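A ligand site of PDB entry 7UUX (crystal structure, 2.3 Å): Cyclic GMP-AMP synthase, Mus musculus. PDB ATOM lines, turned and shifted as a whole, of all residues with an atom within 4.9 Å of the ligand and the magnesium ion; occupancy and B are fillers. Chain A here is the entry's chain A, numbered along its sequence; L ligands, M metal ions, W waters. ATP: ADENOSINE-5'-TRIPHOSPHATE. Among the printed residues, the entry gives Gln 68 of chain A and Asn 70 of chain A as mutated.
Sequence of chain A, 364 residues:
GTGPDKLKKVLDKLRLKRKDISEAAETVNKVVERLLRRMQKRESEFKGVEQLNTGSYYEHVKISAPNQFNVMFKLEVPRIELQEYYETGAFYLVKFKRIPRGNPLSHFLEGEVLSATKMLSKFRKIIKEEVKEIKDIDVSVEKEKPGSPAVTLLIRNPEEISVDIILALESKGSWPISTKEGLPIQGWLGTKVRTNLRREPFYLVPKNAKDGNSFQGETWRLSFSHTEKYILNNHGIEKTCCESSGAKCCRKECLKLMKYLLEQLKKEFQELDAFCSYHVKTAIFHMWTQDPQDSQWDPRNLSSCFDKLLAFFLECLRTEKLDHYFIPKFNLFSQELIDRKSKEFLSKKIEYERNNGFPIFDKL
NZ of Lys 259 is in salt-bridge range of O1G of the ligand.
An oxygen (O2B) of the ligand lies close to the backbone NH (N) of Ser 56 (2.8 Å).
The side-chain amino group (NZ) of Lys 281 is in hydrogen-bond range of an oxygen (O3') of the ligand (3.0 Å).
The side-chain hydroxyl (OG) of Ser 225 is in hydrogen-bond range of an oxygen (O2') of the ligand, at 2.8 Å.
The side-chain hydroxyl (OG) of Ser 277 lies within hydrogen-bond range of an oxygen (O3G) of the ligand (2.8 Å).
The side-chain carboxylate (OE1) of Glu 228 lies within hydrogen-bond range of an oxygen (O2') of the ligand.
OG of Ser 56 is in hydrogen-bond range of O1G of the ligand, at 2.8 Å.
The side-chain carboxylate of Glu 228 lies within salt-bridge range of the side-chain amino group of Lys 281 (2.8 Å).
N of Tyr 278 lies close to SG of Cys 276 (3.7 Å).
OD2 of Asp 164 sits at hydrogen-bond distance from NE2 of Gln 68, at 2.9 Å.
The backbone NH of Lys 62 is in hydrogen-bond range of the backbone carbonyl oxygen of Ser 56, 3.2 Å away.
The side-chain carboxylate (OE2) of Glu 59 lies within salt-bridge range of the side-chain amino group (NZ) of Lys 281 (2.7 Å).
OH of Tyr 278 sits close to NE2 of His 324.
The side-chain carboxylate (OE2) of Glu 228 lies within hydrogen-bond range of the side-chain hydroxyl (OH) of Tyr 278.
CA of Gly 55 touches O2B of the ligand, at 3.4 Å.
Lys 62 touches the ligand.
NH1 of Arg 221 touches C2 of the ligand (3.2 Å).
Tyr 278 touches the ligand.
12 residues have an atom within 4 Å of the ligand: Gly 55, Ser 56, Lys 62, Gln 68, Asn 70, Arg 221, Ser 225, Glu 228, Lys 259, Ser 277, Tyr 278 and Lys 281.
The nearest printed residue that does not touch the ligand is His 324 (4.4 Å).
OG of Ser 56 touches the magnesium ion, at 3.8 Å.
Of the 17 residues printed, 3 come within 4 Å of the magnesium ion.
The magnesium ion is bound by the side-chain amide oxygen (OE1) of Gln 68 (2.1 Å), an oxygen (O2G) of the ligand (2.1 Å), the side-chain amide oxygen (OD1) of Asn 70 (2.1 Å), an oxygen (O2B) of the ligand (2.1 Å), an oxygen (O2A) of the ligand (2.1 Å) and water W2 (2.1 Å).
Water W2 lies within hydrogen-bond range of OG of Ser 56 (2.5 Å) and O of Gln 68 (2.9 Å).
Water W4 lies within hydrogen-bond range of an oxygen (O1B) of the ligand (2.6 Å) and the side-chain carboxylate (OE1) of Glu 59 (2.6 Å).
Water W1 lies within hydrogen-bond range of an oxygen (O1G) of the ligand, the side-chain amino group (NZ) of Lys 62 and the side-chain carboxylate (OE2) of Glu 263.
Water W3 lies within hydrogen-bond range of OG of Ser 277, O1A of the ligand, N of Tyr 278 and SG of Cys 276.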
ATOM      1  N   GLY A  55      -8.199  -1.008   2.286  1.00  0.00           N
ATOM      2  CA  GLY A  55      -9.292  -1.972   2.256  1.00  0.00           C
ATOM      3  C   GLY A  55      -9.778  -2.312   0.880  1.00  0.00           C
ATOM      4  O   GLY A  55      -9.154  -1.927  -0.107  1.00  0.00           O
ATOM      5  N   SER A  56     -10.899  -3.026   0.814  1.00  0.00           N
ATOM      6  CA  SER A  56     -11.251  -3.785  -0.391  1.00  0.00           C
ATOM      7  C   SER A  56     -11.416  -2.918  -1.618  1.00  0.00           C
ATOM      8  O   SER A  56     -11.138  -3.357  -2.722  1.00  0.00           O
ATOM      9  CB  SER A  56     -12.530  -4.605  -0.158  1.00  0.00           C
ATOM     10  OG  SER A  56     -13.661  -3.776   0.115  1.00  0.00           O
ATOM     11  N   GLU A  59      -8.158  -1.992  -3.016  1.00  0.00           N
ATOM     12  CA  GLU A  59      -7.480  -3.210  -3.446  1.00  0.00           C
ATOM     13  C   GLU A  59      -8.148  -3.846  -4.683  1.00  0.00           C
ATOM     14  O   GLU A  59      -7.645  -4.800  -5.223  1.00  0.00           O
ATOM     15  CB  GLU A  59      -7.428  -4.202  -2.285  1.00  0.00           C
ATOM     16  CG  GLU A  59      -6.538  -3.749  -1.106  1.00  0.00           C
ATOM     17  CD  GLU A  59      -6.801  -4.553   0.173  1.00  0.00           C
ATOM     18  OE1 GLU A  59      -7.844  -5.223   0.264  1.00  0.00           O
ATOM     19  OE2 GLU A  59      -5.957  -4.484   1.115  1.00  0.00           O
ATOM     20  N   LYS A  62     -13.529  -5.227  -3.707  1.00  0.00           N
ATOM     21  CA  LYS A  62     -14.843  -4.901  -3.199  1.00  0.00           C
ATOM     22  C   LYS A  62     -15.841  -5.567  -4.120  1.00  0.00           C
ATOM     23  O   LYS A  62     -15.701  -5.508  -5.328  1.00  0.00           O
ATOM     24  CB  LYS A  62     -15.063  -3.385  -3.198  1.00  0.00           C
ATOM     25  CG  LYS A  62     -16.414  -2.930  -2.627  1.00  0.00           C
ATOM     26  CD  LYS A  62     -16.389  -3.009  -1.116  1.00  0.00           C
ATOM     27  CE  LYS A  62     -17.758  -2.770  -0.498  1.00  0.00           C
ATOM     28  NZ  LYS A  62     -18.798  -3.708  -0.971  1.00  0.00           N
ATOM     29  N   GLN A  68     -18.897   0.595   0.720  1.00  0.00           N
ATOM     30  CA  GLN A  68     -18.095   0.578   1.938  1.00  0.00           C
ATOM     31  C   GLN A  68     -16.670   0.906   1.615  1.00  0.00           C
ATOM     32  O   GLN A  68     -16.042   0.232   0.836  1.00  0.00           O
ATOM     33  CB  GLN A  68     -18.169  -0.791   2.640  1.00  0.00           C
ATOM     34  CG  GLN A  68     -18.007  -0.733   4.158  1.00  0.00           C
ATOM     35  CD  GLN A  68     -16.559  -0.842   4.643  1.00  0.00           C
ATOM     36  OE1 GLN A  68     -15.608  -1.090   3.893  1.00  0.00           O
ATOM     37  NE2 GLN A  68     -16.398  -0.713   5.950  1.00  0.00           N
ATOM     38  N   ASN A  70     -12.820   2.377   3.190  1.00  0.00           N
ATOM     39  CA  ASN A  70     -11.959   2.484   4.314  1.00  0.00           C
ATOM     40  C   ASN A  70     -10.915   3.525   4.056  1.00  0.00           C
ATOM     41  O   ASN A  70     -10.327   3.576   2.964  1.00  0.00           O
ATOM     42  CB  ASN A  70     -11.307   1.146   4.607  1.00  0.00           C
ATOM     43  CG  ASN A  70     -12.334   0.049   4.788  1.00  0.00           C
ATOM     44  OD1 ASN A  70     -12.735  -0.612   3.818  1.00  0.00           O
ATOM     45  ND2 ASN A  70     -12.836  -0.083   5.995  1.00  0.00           N
ATOM     46  N   ASP A 164     -15.559   4.199   6.770  1.00  0.00           N
ATOM     47  CA  ASP A 164     -14.870   4.018   8.038  1.00  0.00           C
ATOM     48  C   ASP A 164     -13.607   4.869   8.035  1.00  0.00           C
ATOM     49  O   ASP A 164     -12.696   4.560   7.310  1.00  0.00           O
ATOM     50  CB  ASP A 164     -14.482   2.551   8.260  1.00  0.00           C
ATOM     51  CG  ASP A 164     -15.674   1.628   8.533  1.00  0.00           C
ATOM     52  OD1 ASP A 164     -16.804   2.122   8.770  1.00  0.00           O
ATOM     53  OD2 ASP A 164     -15.449   0.386   8.509  1.00  0.00           O
ATOM     54  N   ARG A 221      -3.657  -1.200  18.786  1.00  0.00           N
ATOM     55  CA  ARG A 221      -3.539  -2.436  17.977  1.00  0.00           C
ATOM     56  C   ARG A 221      -2.729  -2.119  16.704  1.00  0.00           C
ATOM     57  O   ARG A 221      -2.967  -1.049  16.106  1.00  0.00           O
ATOM     58  CB  ARG A 221      -4.936  -3.015  17.670  1.00  0.00           C
ATOM     59  CG  ARG A 221      -4.922  -4.289  16.823  1.00  0.00           C
ATOM     60  CD  ARG A 221      -6.299  -4.859  16.543  1.00  0.00           C
ATOM     61  NE  ARG A 221      -7.212  -3.988  15.826  1.00  0.00           N
ATOM     62  CZ  ARG A 221      -7.116  -3.662  14.522  1.00  0.00           C
ATOM     63  NH1 ARG A 221      -6.109  -4.109  13.790  1.00  0.00           N
ATOM     64  NH2 ARG A 221      -8.025  -2.873  13.967  1.00  0.00           N
ATOM     65  N   SER A 225      -2.623  -2.460   7.038  1.00  0.00           N
ATOM     66  CA  SER A 225      -3.506  -2.162   5.922  1.00  0.00           C
ATOM     67  C   SER A 225      -2.778  -1.660   4.722  1.00  0.00           C
ATOM     68  O   SER A 225      -3.136  -2.017   3.603  1.00  0.00           O
ATOM     69  CB  SER A 225      -4.561  -1.151   6.336  1.00  0.00           C
ATOM     70  OG  SER A 225      -5.549  -1.786   7.104  1.00  0.00           O
ATOM     71  N   GLU A 228      -0.865  -4.637   3.243  1.00  0.00           N
ATOM     72  CA  GLU A 228      -1.813  -5.529   2.623  1.00  0.00           C
ATOM     73  C   GLU A 228      -2.255  -5.009   1.253  1.00  0.00           C
ATOM     74  O   GLU A 228      -2.440  -5.790   0.306  1.00  0.00           O
ATOM     75  CB  GLU A 228      -3.035  -5.714   3.542  1.00  0.00           C
ATOM     76  CG  GLU A 228      -2.721  -6.402   4.850  1.00  0.00           C
ATOM     77  CD  GLU A 228      -3.836  -6.333   5.867  1.00  0.00           C
ATOM     78  OE1 GLU A 228      -4.953  -5.850   5.553  1.00  0.00           O
ATOM     79  OE2 GLU A 228      -3.562  -6.750   6.992  1.00  0.00           O
ATOM     80  N   LYS A 259     -15.078 -14.081  -0.078  1.00  0.00           N
ATOM     81  CA  LYS A 259     -15.690 -12.911   0.546  1.00  0.00           C
ATOM     82  C   LYS A 259     -17.215 -12.968   0.452  1.00  0.00           C
ATOM     83  O   LYS A 259     -17.906 -12.735   1.449  1.00  0.00           O
ATOM     84  CB  LYS A 259     -15.191 -11.596  -0.084  1.00  0.00           C
ATOM     85  CG  LYS A 259     -13.885 -11.092   0.489  1.00  0.00           C
ATOM     86  CD  LYS A 259     -13.235 -10.023  -0.363  1.00  0.00           C
ATOM     87  CE  LYS A 259     -13.996  -8.709  -0.326  1.00  0.00           C
ATOM     88  NZ  LYS A 259     -13.946  -8.065   1.008  1.00  0.00           N
ATOM     89  N   GLU A 263     -20.092 -13.134   3.321  1.00  0.00           N
ATOM     90  CA  GLU A 263     -21.145 -12.069   3.364  1.00  0.00           C
ATOM     91  C   GLU A 263     -22.581 -12.626   3.314  1.00  0.00           C
ATOM     92  O   GLU A 263     -23.438 -12.252   4.105  1.00  0.00           O
ATOM     93  CB  GLU A 263     -20.992 -11.042   2.227  1.00  0.00           C
ATOM     94  CG  GLU A 263     -19.942  -9.947   2.441  1.00  0.00           C
ATOM     95  CD  GLU A 263     -19.906  -8.892   1.315  1.00  0.00           C
ATOM     96  OE1 GLU A 263     -20.973  -8.577   0.748  1.00  0.00           O
ATOM     97  OE2 GLU A 263     -18.810  -8.357   0.996  1.00  0.00           O
ATOM     98  N   CYS A 276     -15.543 -12.087  10.129  1.00  0.00           N
ATOM     99  CA  CYS A 276     -15.457 -10.925   9.273  1.00  0.00           C
ATOM    100  C   CYS A 276     -14.594 -11.229   8.075  1.00  0.00           C
ATOM    101  O   CYS A 276     -13.898 -12.246   8.030  1.00  0.00           O
ATOM    102  CB  CYS A 276     -14.901  -9.720  10.046  1.00  0.00           C
ATOM    103  SG  CYS A 276     -13.219  -9.955  10.587  1.00  0.00           S
ATOM    104  N   SER A 277     -14.615 -10.331   7.095  1.00  0.00           N
ATOM    105  CA  SER A 277     -13.871 -10.531   5.887  1.00  0.00           C
ATOM    106  C   SER A 277     -12.356 -10.603   6.100  1.00  0.00           C
ATOM    107  O   SER A 277     -11.616 -11.202   5.276  1.00  0.00           O
ATOM    108  CB  SER A 277     -14.253  -9.474   4.854  1.00  0.00           C
ATOM    109  OG  SER A 277     -13.894  -8.184   5.283  1.00  0.00           O
ATOM    110  N   TYR A 278     -11.844 -10.057   7.206  1.00  0.00           N
ATOM    111  CA  TYR A 278     -10.389 -10.101   7.468  1.00  0.00           C
ATOM    112  C   TYR A 278      -9.960 -11.570   7.660  1.00  0.00           C
ATOM    113  O   TYR A 278      -8.781 -11.917   7.404  1.00  0.00           O
ATOM    114  CB  TYR A 278      -9.971  -9.220   8.656  1.00  0.00           C
ATOM    115  CG  TYR A 278      -8.471  -9.040   8.724  1.00  0.00           C
ATOM    116  CD1 TYR A 278      -7.809  -8.339   7.735  1.00  0.00           C
ATOM    117  CD2 TYR A 278      -7.694  -9.591   9.741  1.00  0.00           C
ATOM    118  CE1 TYR A 278      -6.427  -8.160   7.759  1.00  0.00           C
ATOM    119  CE2 TYR A 278      -6.316  -9.439   9.775  1.00  0.00           C
ATOM    120  CZ  TYR A 278      -5.672  -8.722   8.780  1.00  0.00           C
ATOM    121  OH  TYR A 278      -4.309  -8.544   8.758  1.00  0.00           O
ATOM    122  N   LYS A 281      -9.363 -12.890   4.181  1.00  0.00           N
ATOM    123  CA  LYS A 281      -8.195 -12.190   3.622  1.00  0.00           C
ATOM    124  C   LYS A 281      -6.891 -12.802   4.160  1.00  0.00           C
ATOM    125  O   LYS A 281      -5.982 -13.135   3.414  1.00  0.00           O
ATOM    126  CB  LYS A 281      -8.289 -10.683   3.938  1.00  0.00           C
ATOM    127  CG  LYS A 281      -7.351  -9.790   3.145  1.00  0.00           C
ATOM    128  CD  LYS A 281      -7.505  -8.326   3.569  1.00  0.00           C
ATOM    129  CE  LYS A 281      -6.668  -7.378   2.725  1.00  0.00           C
ATOM    130  NZ  LYS A 281      -6.564  -5.978   3.286  1.00  0.00           N
ATOM    131  N   HIS A 324      -2.546 -14.511  12.402  1.00  0.00           N
ATOM    132  CA  HIS A 324      -2.352 -13.217  11.767  1.00  0.00           C
ATOM    133  C   HIS A 324      -1.089 -13.342  10.893  1.00  0.00           C
ATOM    134  O   HIS A 324      -0.096 -13.904  11.313  1.00  0.00           O
ATOM    135  CB  HIS A 324      -2.181 -12.157  12.856  1.00  0.00           C
ATOM    136  CG  HIS A 324      -2.384 -10.757  12.371  1.00  0.00           C
ATOM    137  ND1 HIS A 324      -1.557 -10.168  11.447  1.00  0.00           N
ATOM    138  CD2 HIS A 324      -3.325  -9.831  12.703  1.00  0.00           C
ATOM    139  CE1 HIS A 324      -1.962  -8.929  11.223  1.00  0.00           C
ATOM    140  NE2 HIS A 324      -3.026  -8.698  11.987  1.00  0.00           N
HETATM  141  PG  ATP L   1     -14.846  -5.485   2.904  1.00  0.00           P
HETATM  142  O1G ATP L   1     -15.139  -5.687   1.443  1.00  0.00           O
HETATM  143  O2G ATP L   1     -15.053  -4.040   3.335  1.00  0.00           O
HETATM  144  O3G ATP L   1     -15.549  -6.489   3.769  1.00  0.00           O
HETATM  145  PB  ATP L   1     -12.074  -4.855   3.749  1.00  0.00           P
HETATM  146  O1B ATP L   1     -10.757  -5.551   3.530  1.00  0.00           O
HETATM  147  O2B ATP L   1     -12.226  -3.448   3.261  1.00  0.00           O
HETATM  148  O3B ATP L   1     -13.245  -5.757   3.126  1.00  0.00           O
HETATM  149  PA  ATP L   1     -13.018  -3.872   6.382  1.00  0.00           P
HETATM  150  O1A ATP L   1     -13.828  -4.627   7.378  1.00  0.00           O
HETATM  151  O2A ATP L   1     -13.688  -2.761   5.640  1.00  0.00           O
HETATM  152  O3A ATP L   1     -12.441  -4.911   5.298  1.00  0.00           O
HETATM  153  O5' ATP L   1     -11.676  -3.352   7.108  1.00  0.00           O
HETATM  154  C5' ATP L   1     -10.666  -2.596   6.384  1.00  0.00           C
HETATM  155  C4' ATP L   1      -9.279  -3.093   6.717  1.00  0.00           C
HETATM  156  O4' ATP L   1      -9.086  -3.069   8.157  1.00  0.00           O
HETATM  157  C3' ATP L   1      -8.953  -4.545   6.326  1.00  0.00           C
HETATM  158  O3' ATP L   1      -8.633  -4.647   4.945  1.00  0.00           O
HETATM  159  C2' ATP L   1      -7.782  -4.855   7.278  1.00  0.00           C
HETATM  160  O2' ATP L   1      -6.511  -4.418   6.867  1.00  0.00           O
HETATM  161  C1' ATP L   1      -8.222  -4.122   8.549  1.00  0.00           C
HETATM  162  N9  ATP L   1      -8.933  -5.000   9.479  1.00  0.00           N
HETATM  163  C8  ATP L   1     -10.280  -5.289   9.498  1.00  0.00           C
HETATM  164  N7  ATP L   1     -10.594  -6.124  10.463  1.00  0.00           N
HETATM  165  C5  ATP L   1      -9.385  -6.414  11.088  1.00  0.00           C
HETATM  166  C6  ATP L   1      -9.049  -7.241  12.184  1.00  0.00           C
HETATM  167  N6  ATP L   1      -9.933  -7.975  12.853  1.00  0.00           N
HETATM  168  N1  ATP L   1      -7.740  -7.294  12.549  1.00  0.00           N
HETATM  169  C2  ATP L   1      -6.846  -6.562  11.858  1.00  0.00           C
HETATM  170  N3  ATP L   1      -7.056  -5.752  10.821  1.00  0.00           N
HETATM  171  C4  ATP L   1      -8.357  -5.712  10.484  1.00  0.00           C
HETATM  172 MG    MG M   1     -13.956  -2.290   3.597  1.00  0.00          MG
HETATM  173  O   HOH W   1     -17.185  -6.117  -0.241  1.00  0.00           O
HETATM  174  O   HOH W   2     -14.103  -1.735   1.559  1.00  0.00           O
HETATM  175  O   HOH W   3     -13.277  -7.503   8.066  1.00  0.00           O
HETATM  176  O   HOH W   4      -9.781  -6.576   1.406  1.00  0.00           O
